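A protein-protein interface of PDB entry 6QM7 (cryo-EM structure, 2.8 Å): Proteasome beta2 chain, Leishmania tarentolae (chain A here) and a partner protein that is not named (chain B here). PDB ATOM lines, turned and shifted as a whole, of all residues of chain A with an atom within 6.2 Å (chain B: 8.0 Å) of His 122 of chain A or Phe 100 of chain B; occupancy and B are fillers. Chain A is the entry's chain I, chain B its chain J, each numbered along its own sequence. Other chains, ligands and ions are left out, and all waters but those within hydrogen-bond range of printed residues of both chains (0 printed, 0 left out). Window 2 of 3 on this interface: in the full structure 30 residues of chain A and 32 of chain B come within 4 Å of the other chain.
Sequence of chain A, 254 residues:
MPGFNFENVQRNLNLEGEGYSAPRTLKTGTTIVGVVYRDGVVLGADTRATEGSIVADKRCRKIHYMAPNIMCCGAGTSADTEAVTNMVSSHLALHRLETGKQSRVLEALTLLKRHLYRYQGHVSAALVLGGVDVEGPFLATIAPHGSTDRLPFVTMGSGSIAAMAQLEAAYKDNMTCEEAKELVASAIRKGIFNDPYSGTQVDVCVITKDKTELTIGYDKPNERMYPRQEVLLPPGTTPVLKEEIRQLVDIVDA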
ATOM      1  N   THR A  77      32.524  25.310 -37.342  1.00  0.00           N
ATOM      2  CA  THR A  77      33.415  24.522 -36.453  1.00  0.00           C
ATOM      3  C   THR A  77      33.407  23.077 -36.949  1.00  0.00           C
ATOM      4  O   THR A  77      32.322  22.478 -36.915  1.00  0.00           O
ATOM      5  CB  THR A  77      32.960  24.680 -34.996  1.00  0.00           C
ATOM      6  OG1 THR A  77      32.972  26.069 -34.669  1.00  0.00           O
ATOM      7  CG2 THR A  77      33.824  23.928 -34.012  1.00  0.00           C
ATOM      8  N   ASP A  80      31.907  20.309 -34.817  1.00  0.00           N
ATOM      9  CA  ASP A  80      30.438  20.428 -34.639  1.00  0.00           C
ATOM     10  C   ASP A  80      29.740  19.920 -35.892  1.00  0.00           C
ATOM     11  O   ASP A  80      28.813  19.129 -35.778  1.00  0.00           O
ATOM     12  CB  ASP A  80      30.048  21.877 -34.363  1.00  0.00           C
ATOM     13  CG  ASP A  80      30.372  22.320 -32.948  1.00  0.00           C
ATOM     14  OD1 ASP A  80      30.036  21.567 -32.004  1.00  0.00           O
ATOM     15  OD2 ASP A  80      30.934  23.426 -32.796  1.00  0.00           O
ATOM     16  N   LEU A 116      20.582  22.001 -33.608  1.00  0.00           N
ATOM     17  CA  LEU A 116      21.341  23.270 -33.634  1.00  0.00           C
ATOM     18  C   LEU A 116      20.612  24.336 -32.835  1.00  0.00           C
ATOM     19  O   LEU A 116      21.318  25.060 -32.134  1.00  0.00           O
ATOM     20  CB  LEU A 116      21.535  23.716 -35.077  1.00  0.00           C
ATOM     21  CG  LEU A 116      22.490  22.836 -35.864  1.00  0.00           C
ATOM     22  CD1 LEU A 116      22.613  23.353 -37.291  1.00  0.00           C
ATOM     23  CD2 LEU A 116      23.849  22.746 -35.165  1.00  0.00           C
ATOM     24  N   TYR A 119      21.063  24.263 -28.981  1.00  0.00           N
ATOM     25  CA  TYR A 119      22.405  24.674 -28.488  1.00  0.00           C
ATOM     26  C   TYR A 119      22.702  26.150 -28.792  1.00  0.00           C
ATOM     27  O   TYR A 119      23.851  26.569 -28.564  1.00  0.00           O
ATOM     28  CB  TYR A 119      23.480  23.719 -29.016  1.00  0.00           C
ATOM     29  CG  TYR A 119      23.418  22.373 -28.343  1.00  0.00           C
ATOM     30  CD1 TYR A 119      23.891  22.197 -27.050  1.00  0.00           C
ATOM     31  CD2 TYR A 119      22.808  21.295 -28.961  1.00  0.00           C
ATOM     32  CE1 TYR A 119      23.788  20.976 -26.404  1.00  0.00           C
ATOM     33  CE2 TYR A 119      22.694  20.068 -28.328  1.00  0.00           C
ATOM     34  CZ  TYR A 119      23.187  19.905 -27.047  1.00  0.00           C
ATOM     35  OH  TYR A 119      23.081  18.690 -26.437  1.00  0.00           O
ATOM     36  N   GLN A 120      21.708  26.921 -29.239  1.00  0.00           N
ATOM     37  CA  GLN A 120      21.745  28.408 -29.309  1.00  0.00           C
ATOM     38  C   GLN A 120      22.970  28.884 -30.102  1.00  0.00           C
ATOM     39  O   GLN A 120      23.481  29.961 -29.789  1.00  0.00           O
ATOM     40  CB  GLN A 120      21.748  29.014 -27.897  1.00  0.00           C
ATOM     41  CG  GLN A 120      20.680  28.476 -26.937  1.00  0.00           C
ATOM     42  CD  GLN A 120      19.259  28.691 -27.406  1.00  0.00           C
ATOM     43  OE1 GLN A 120      18.942  29.617 -28.155  1.00  0.00           O
ATOM     44  NE2 GLN A 120      18.371  27.814 -26.965  1.00  0.00           N
ATOM     45  N   GLY A 121      23.427  28.117 -31.091  1.00  0.00           N
ATOM     46  CA  GLY A 121      24.575  28.482 -31.944  1.00  0.00           C
ATOM     47  C   GLY A 121      25.929  28.104 -31.354  1.00  0.00           C
ATOM     48  O   GLY A 121      26.947  28.365 -32.031  1.00  0.00           O
ATOM     49  N   HIS A 122      25.969  27.510 -30.160  1.00  0.00           N
ATOM     50  CA  HIS A 122      27.231  27.090 -29.501  1.00  0.00           C
ATOM     51  C   HIS A 122      27.778  25.863 -30.225  1.00  0.00           C
ATOM     52  O   HIS A 122      29.018  25.722 -30.264  1.00  0.00           O
ATOM     53  CB  HIS A 122      27.038  26.891 -27.993  1.00  0.00           C
ATOM     54  CG  HIS A 122      26.598  28.136 -27.303  1.00  0.00           C
ATOM     55  ND1 HIS A 122      27.082  29.382 -27.671  1.00  0.00           N
ATOM     56  CD2 HIS A 122      25.698  28.337 -26.313  1.00  0.00           C
ATOM     57  CE1 HIS A 122      26.505  30.301 -26.930  1.00  0.00           C
ATOM     58  NE2 HIS A 122      25.648  29.684 -26.087  1.00  0.00           N
ATOM     59  N   VAL A 123      26.895  25.019 -30.766  1.00  0.00           N
ATOM     60  CA  VAL A 123      27.236  24.026 -31.821  1.00  0.00           C
ATOM     61  C   VAL A 123      27.209  24.795 -33.132  1.00  0.00           C
ATOM     62  O   VAL A 123      26.115  24.983 -33.668  1.00  0.00           O
ATOM     63  CB  VAL A 123      26.281  22.822 -31.830  1.00  0.00           C
ATOM     64  CG1 VAL A 123      26.553  21.876 -32.993  1.00  0.00           C
ATOM     65  CG2 VAL A 123      26.340  22.065 -30.514  1.00  0.00           C
ATOM     66  N   SER A 124      28.374  25.255 -33.586  1.00  0.00           N
ATOM     67  CA  SER A 124      28.515  26.256 -34.669  1.00  0.00           C
ATOM     68  C   SER A 124      28.703  25.549 -36.017  1.00  0.00           C
ATOM     69  O   SER A 124      29.648  25.898 -36.759  1.00  0.00           O
ATOM     70  CB  SER A 124      29.633  27.219 -34.365  1.00  0.00           C
ATOM     71  OG  SER A 124      29.893  28.061 -35.483  1.00  0.00           O
ATOM     72  N   PRO A 144      23.946  27.981 -37.945  1.00  0.00           N
ATOM     73  CA  PRO A 144      24.297  27.479 -36.616  1.00  0.00           C
ATOM     74  C   PRO A 144      23.242  27.640 -35.510  1.00  0.00           C
ATOM     75  O   PRO A 144      23.187  26.811 -34.635  1.00  0.00           O
ATOM     76  CB  PRO A 144      25.473  28.381 -36.239  1.00  0.00           C
ATOM     77  CG  PRO A 144      26.113  28.686 -37.560  1.00  0.00           C
ATOM     78  CD  PRO A 144      24.937  28.928 -38.468  1.00  0.00           C
ATOM     79  N   HIS A 145      22.467  28.719 -35.569  1.00  0.00           N
ATOM     80  CA  HIS A 145      21.377  29.020 -34.613  1.00  0.00           C
ATOM     81  C   HIS A 145      20.137  28.186 -34.921  1.00  0.00           C
ATOM     82  O   HIS A 145      19.220  28.252 -34.103  1.00  0.00           O
ATOM     83  CB  HIS A 145      21.060  30.518 -34.614  1.00  0.00           C
ATOM     84  CG  HIS A 145      22.110  31.327 -33.944  1.00  0.00           C
ATOM     85  ND1 HIS A 145      23.194  31.832 -34.639  1.00  0.00           N
ATOM     86  CD2 HIS A 145      22.271  31.682 -32.651  1.00  0.00           C
ATOM     87  CE1 HIS A 145      23.982  32.476 -33.799  1.00  0.00           C
ATOM     88  NE2 HIS A 145      23.434  32.398 -32.569  1.00  0.00           N
ATOM     89  N   LEU B  95      36.593  13.577 -27.005  1.00  0.00           N
ATOM     90  CA  LEU B  95      36.924  15.017 -26.935  1.00  0.00           C
ATOM     91  C   LEU B  95      35.645  15.834 -27.101  1.00  0.00           C
ATOM     92  O   LEU B  95      35.492  16.822 -26.376  1.00  0.00           O
ATOM     93  CB  LEU B  95      37.954  15.380 -28.002  1.00  0.00           C
ATOM     94  CG  LEU B  95      39.354  14.848 -27.739  1.00  0.00           C
ATOM     95  CD1 LEU B  95      40.216  14.946 -28.977  1.00  0.00           C
ATOM     96  CD2 LEU B  95      40.004  15.568 -26.581  1.00  0.00           C
ATOM     97  N   TYR B  96      34.763  15.427 -28.005  1.00  0.00           N
ATOM     98  CA  TYR B  96      33.481  16.118 -28.279  1.00  0.00           C
ATOM     99  C   TYR B  96      32.473  15.877 -27.151  1.00  0.00           C
ATOM    100  O   TYR B  96      31.567  16.707 -27.008  1.00  0.00           O
ATOM    101  CB  TYR B  96      32.917  15.683 -29.630  1.00  0.00           C
ATOM    102  CG  TYR B  96      31.859  16.623 -30.121  1.00  0.00           C
ATOM    103  CD1 TYR B  96      32.187  17.811 -30.753  1.00  0.00           C
ATOM    104  CD2 TYR B  96      30.524  16.355 -29.879  1.00  0.00           C
ATOM    105  CE1 TYR B  96      31.206  18.695 -31.175  1.00  0.00           C
ATOM    106  CE2 TYR B  96      29.531  17.235 -30.274  1.00  0.00           C
ATOM    107  CZ  TYR B  96      29.871  18.411 -30.921  1.00  0.00           C
ATOM    108  OH  TYR B  96      28.863  19.252 -31.292  1.00  0.00           O
ATOM    109  N   GLU B  97      32.607  14.798 -26.370  1.00  0.00           N
ATOM    110  CA  GLU B  97      31.842  14.602 -25.105  1.00  0.00           C
ATOM    111  C   GLU B  97      32.054  15.817 -24.201  1.00  0.00           C
ATOM    112  O   GLU B  97      31.197  16.055 -23.337  1.00  0.00           O
ATOM    113  CB  GLU B  97      32.272  13.356 -24.324  1.00  0.00           C
ATOM    114  CG  GLU B  97      31.448  12.110 -24.607  1.00  0.00           C
ATOM    115  CD  GLU B  97      31.681  10.947 -23.638  1.00  0.00           C
ATOM    116  OE1 GLU B  97      30.836  10.755 -22.726  1.00  0.00           O
ATOM    117  OE2 GLU B  97      32.697  10.217 -23.802  1.00  0.00           O
ATOM    118  N   ALA B  98      33.162  16.532 -24.379  1.00  0.00           N
ATOM    119  CA  ALA B  98      33.547  17.690 -23.553  1.00  0.00           C
ATOM    120  C   ALA B  98      33.531  18.999 -24.361  1.00  0.00           C
ATOM    121  O   ALA B  98      34.244  19.917 -23.981  1.00  0.00           O
ATOM    122  CB  ALA B  98      34.908  17.398 -22.969  1.00  0.00           C
ATOM    123  N   ARG B  99      32.706  19.115 -25.396  1.00  0.00           N
ATOM    124  CA  ARG B  99      32.648  20.317 -26.277  1.00  0.00           C
ATOM    125  C   ARG B  99      32.611  21.615 -25.468  1.00  0.00           C
ATOM    126  O   ARG B  99      33.315  22.576 -25.841  1.00  0.00           O
ATOM    127  CB  ARG B  99      31.374  20.320 -27.124  1.00  0.00           C
ATOM    128  CG  ARG B  99      31.635  20.289 -28.615  1.00  0.00           C
ATOM    129  CD  ARG B  99      31.494  21.603 -29.341  1.00  0.00           C
ATOM    130  NE  ARG B  99      32.306  22.670 -28.819  1.00  0.00           N
ATOM    131  CZ  ARG B  99      32.351  23.885 -29.341  1.00  0.00           C
ATOM    132  NH1 ARG B  99      31.625  24.191 -30.403  1.00  0.00           N
ATOM    133  NH2 ARG B  99      33.134  24.800 -28.795  1.00  0.00           N
ATOM    134  N   PHE B 100      31.747  21.649 -24.458  1.00  0.00           N
ATOM    135  CA  PHE B 100      31.514  22.804 -23.562  1.00  0.00           C
ATOM    136  C   PHE B 100      32.192  22.458 -22.239  1.00  0.00           C
ATOM    137  O   PHE B 100      31.572  21.768 -21.396  1.00  0.00           O
ATOM    138  CB  PHE B 100      30.012  23.085 -23.469  1.00  0.00           C
ATOM    139  CG  PHE B 100      29.327  23.062 -24.813  1.00  0.00           C
ATOM    140  CD1 PHE B 100      29.587  24.049 -25.757  1.00  0.00           C
ATOM    141  CD2 PHE B 100      28.476  22.018 -25.159  1.00  0.00           C
ATOM    142  CE1 PHE B 100      28.993  24.002 -27.010  1.00  0.00           C
ATOM    143  CE2 PHE B 100      27.878  21.976 -26.412  1.00  0.00           C
ATOM    144  CZ  PHE B 100      28.135  22.971 -27.331  1.00  0.00           C
ATOM    145  N   GLY B 101      33.447  22.896 -22.098  1.00  0.00           N
ATOM    146  CA  GLY B 101      34.392  22.451 -21.052  1.00  0.00           C
ATOM    147  C   GLY B 101      35.346  21.380 -21.570  1.00  0.00           C
ATOM    148  O   GLY B 101      35.336  20.262 -21.062  1.00  0.00           O
ATOM    149  N   PRO B 102      36.210  21.702 -22.562  1.00  0.00           N
ATOM    150  CA  PRO B 102      37.028  20.698 -23.237  1.00  0.00           C
ATOM    151  C   PRO B 102      38.290  20.291 -22.471  1.00  0.00           C
ATOM    152  O   PRO B 102      38.671  20.983 -21.558  1.00  0.00           O
ATOM    153  CB  PRO B 102      37.374  21.393 -24.561  1.00  0.00           C
ATOM    154  CG  PRO B 102      37.493  22.844 -24.186  1.00  0.00           C
ATOM    155  CD  PRO B 102      36.460  23.050 -23.097  1.00  0.00           C
ATOM    156  N   TRP B 103      38.848  19.145 -22.854  1.00  0.00           N
ATOM    157  CA  TRP B 103      40.211  18.698 -22.493  1.00  0.00           C
ATOM    158  C   TRP B 103      41.174  19.560 -23.283  1.00  0.00           C
ATOM    159  O   TRP B 103      41.034  19.579 -24.496  1.00  0.00           O
ATOM    160  CB  TRP B 103      40.437  17.224 -22.844  1.00  0.00           C
ATOM    161  CG  TRP B 103      39.498  16.295 -22.151  1.00  0.00           C
ATOM    162  CD1 TRP B 103      38.445  15.625 -22.691  1.00  0.00           C
ATOM    163  CD2 TRP B 103      39.522  15.964 -20.760  1.00  0.00           C
ATOM    164  NE1 TRP B 103      37.810  14.894 -21.728  1.00  0.00           N
ATOM    165  CE2 TRP B 103      38.448  15.080 -20.533  1.00  0.00           C
ATOM    166  CE3 TRP B 103      40.347  16.332 -19.689  1.00  0.00           C
ATOM    167  CZ2 TRP B 103      38.173  14.560 -19.272  1.00  0.00           C
ATOM    168  CZ3 TRP B 103      40.082  15.817 -18.443  1.00  0.00           C
ATOM    169  CH2 TRP B 103      39.009  14.941 -18.241  1.00  0.00           C
ATOM    170  N   ILE B 127      38.348  19.779 -29.345  1.00  0.00           N
ATOM    171  CA  ILE B 127      36.921  19.353 -29.356  1.00  0.00           C
ATOM    172  C   ILE B 127      36.692  18.277 -30.420  1.00  0.00           C
ATOM    173  O   ILE B 127      35.543  18.101 -30.836  1.00  0.00           O
ATOM    174  CB  ILE B 127      35.984  20.561 -29.536  1.00  0.00           C
ATOM    175  CG1 ILE B 127      36.327  21.403 -30.767  1.00  0.00           C
ATOM    176  CG2 ILE B 127      35.951  21.407 -28.272  1.00  0.00           C
ATOM    177  CD1 ILE B 127      35.211  22.335 -31.190  1.00  0.00           C
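OD1 of Asp 80 of chain A lies within hydrogen-bond range of OH of Tyr 96 of chain B (2.7 Å). The guanidinium group of Arg 99 of chain B is in salt-bridge range of the side-chain carboxylate of Asp 80 of chain A (2.6 Å). The guanidinium group (NH1) of Arg 99 of chain B lies within hydrogen-bond range of the backbone carbonyl oxygen (O) of His 122 of chain A, at 3.0 Å.
N of Thr 77 of chain A sits at hydrogen-bond distance from O of Ser 124 of chain A, 3.0 Å away. The backbone NH of Ser 124 of chain A lies within hydrogen-bond range of the side-chain carboxylate of Asp 80 of chain A (3.2 Å).
Among the printed residues, pairs that only touch across the chains: Thr 77 of chain A with Ile 127 of chain B (3.5 Å), His 122 of chain A with Phe 100 of chain B (3.6 Å), Val 123 of chain A with Tyr 96 of chain B (3.9 Å) and Val 123 of chain A with Phe 100 of chain B (3.8 Å).
His 122 of chain A touches two residues of chain B. Of chain A, only His 122 (3.6 Å) and Val 123 (3.8 Å) come within 4 Å of Phe 100 of chain B. Printed residues of chain A within 4 Å of Tyr 96 of chain B: Asp 80 and Val 123. Printed residues of chain A within 4 Å of Arg 99 of chain B: Asp 80 and His 122. Tyr 119 of chain A touches none of the printed residues of chain B. The nearest residue of chain A that does not touch Phe 100 of chain B is Tyr 119 of chain A (4.04 Å). The nearest printed residue of chain B that does not touch Asp 80 of chain A is Ile 127 of chain B (4.7 Å).
Of the 11 printed residues of chain A, 4 touch a printed residue of chain B. Hydrophobic or aromatic side chains of chain A within 4 Å of the printed part of chain B: His 122 and Val 123. Of the 10 printed residues of chain B, 4 touch a printed residue of chain A. Printed residues of chain B that touch a printed residue of chain A: Tyr 96, Arg 99, Phe 100 and Ile 127. Hydrophobic or aromatic side chains of chain B within 4 Å of the printed part of chain A: Tyr 96, Phe 100 and Ile 127. Among the printed residues, 7 pairs touch across the chains.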
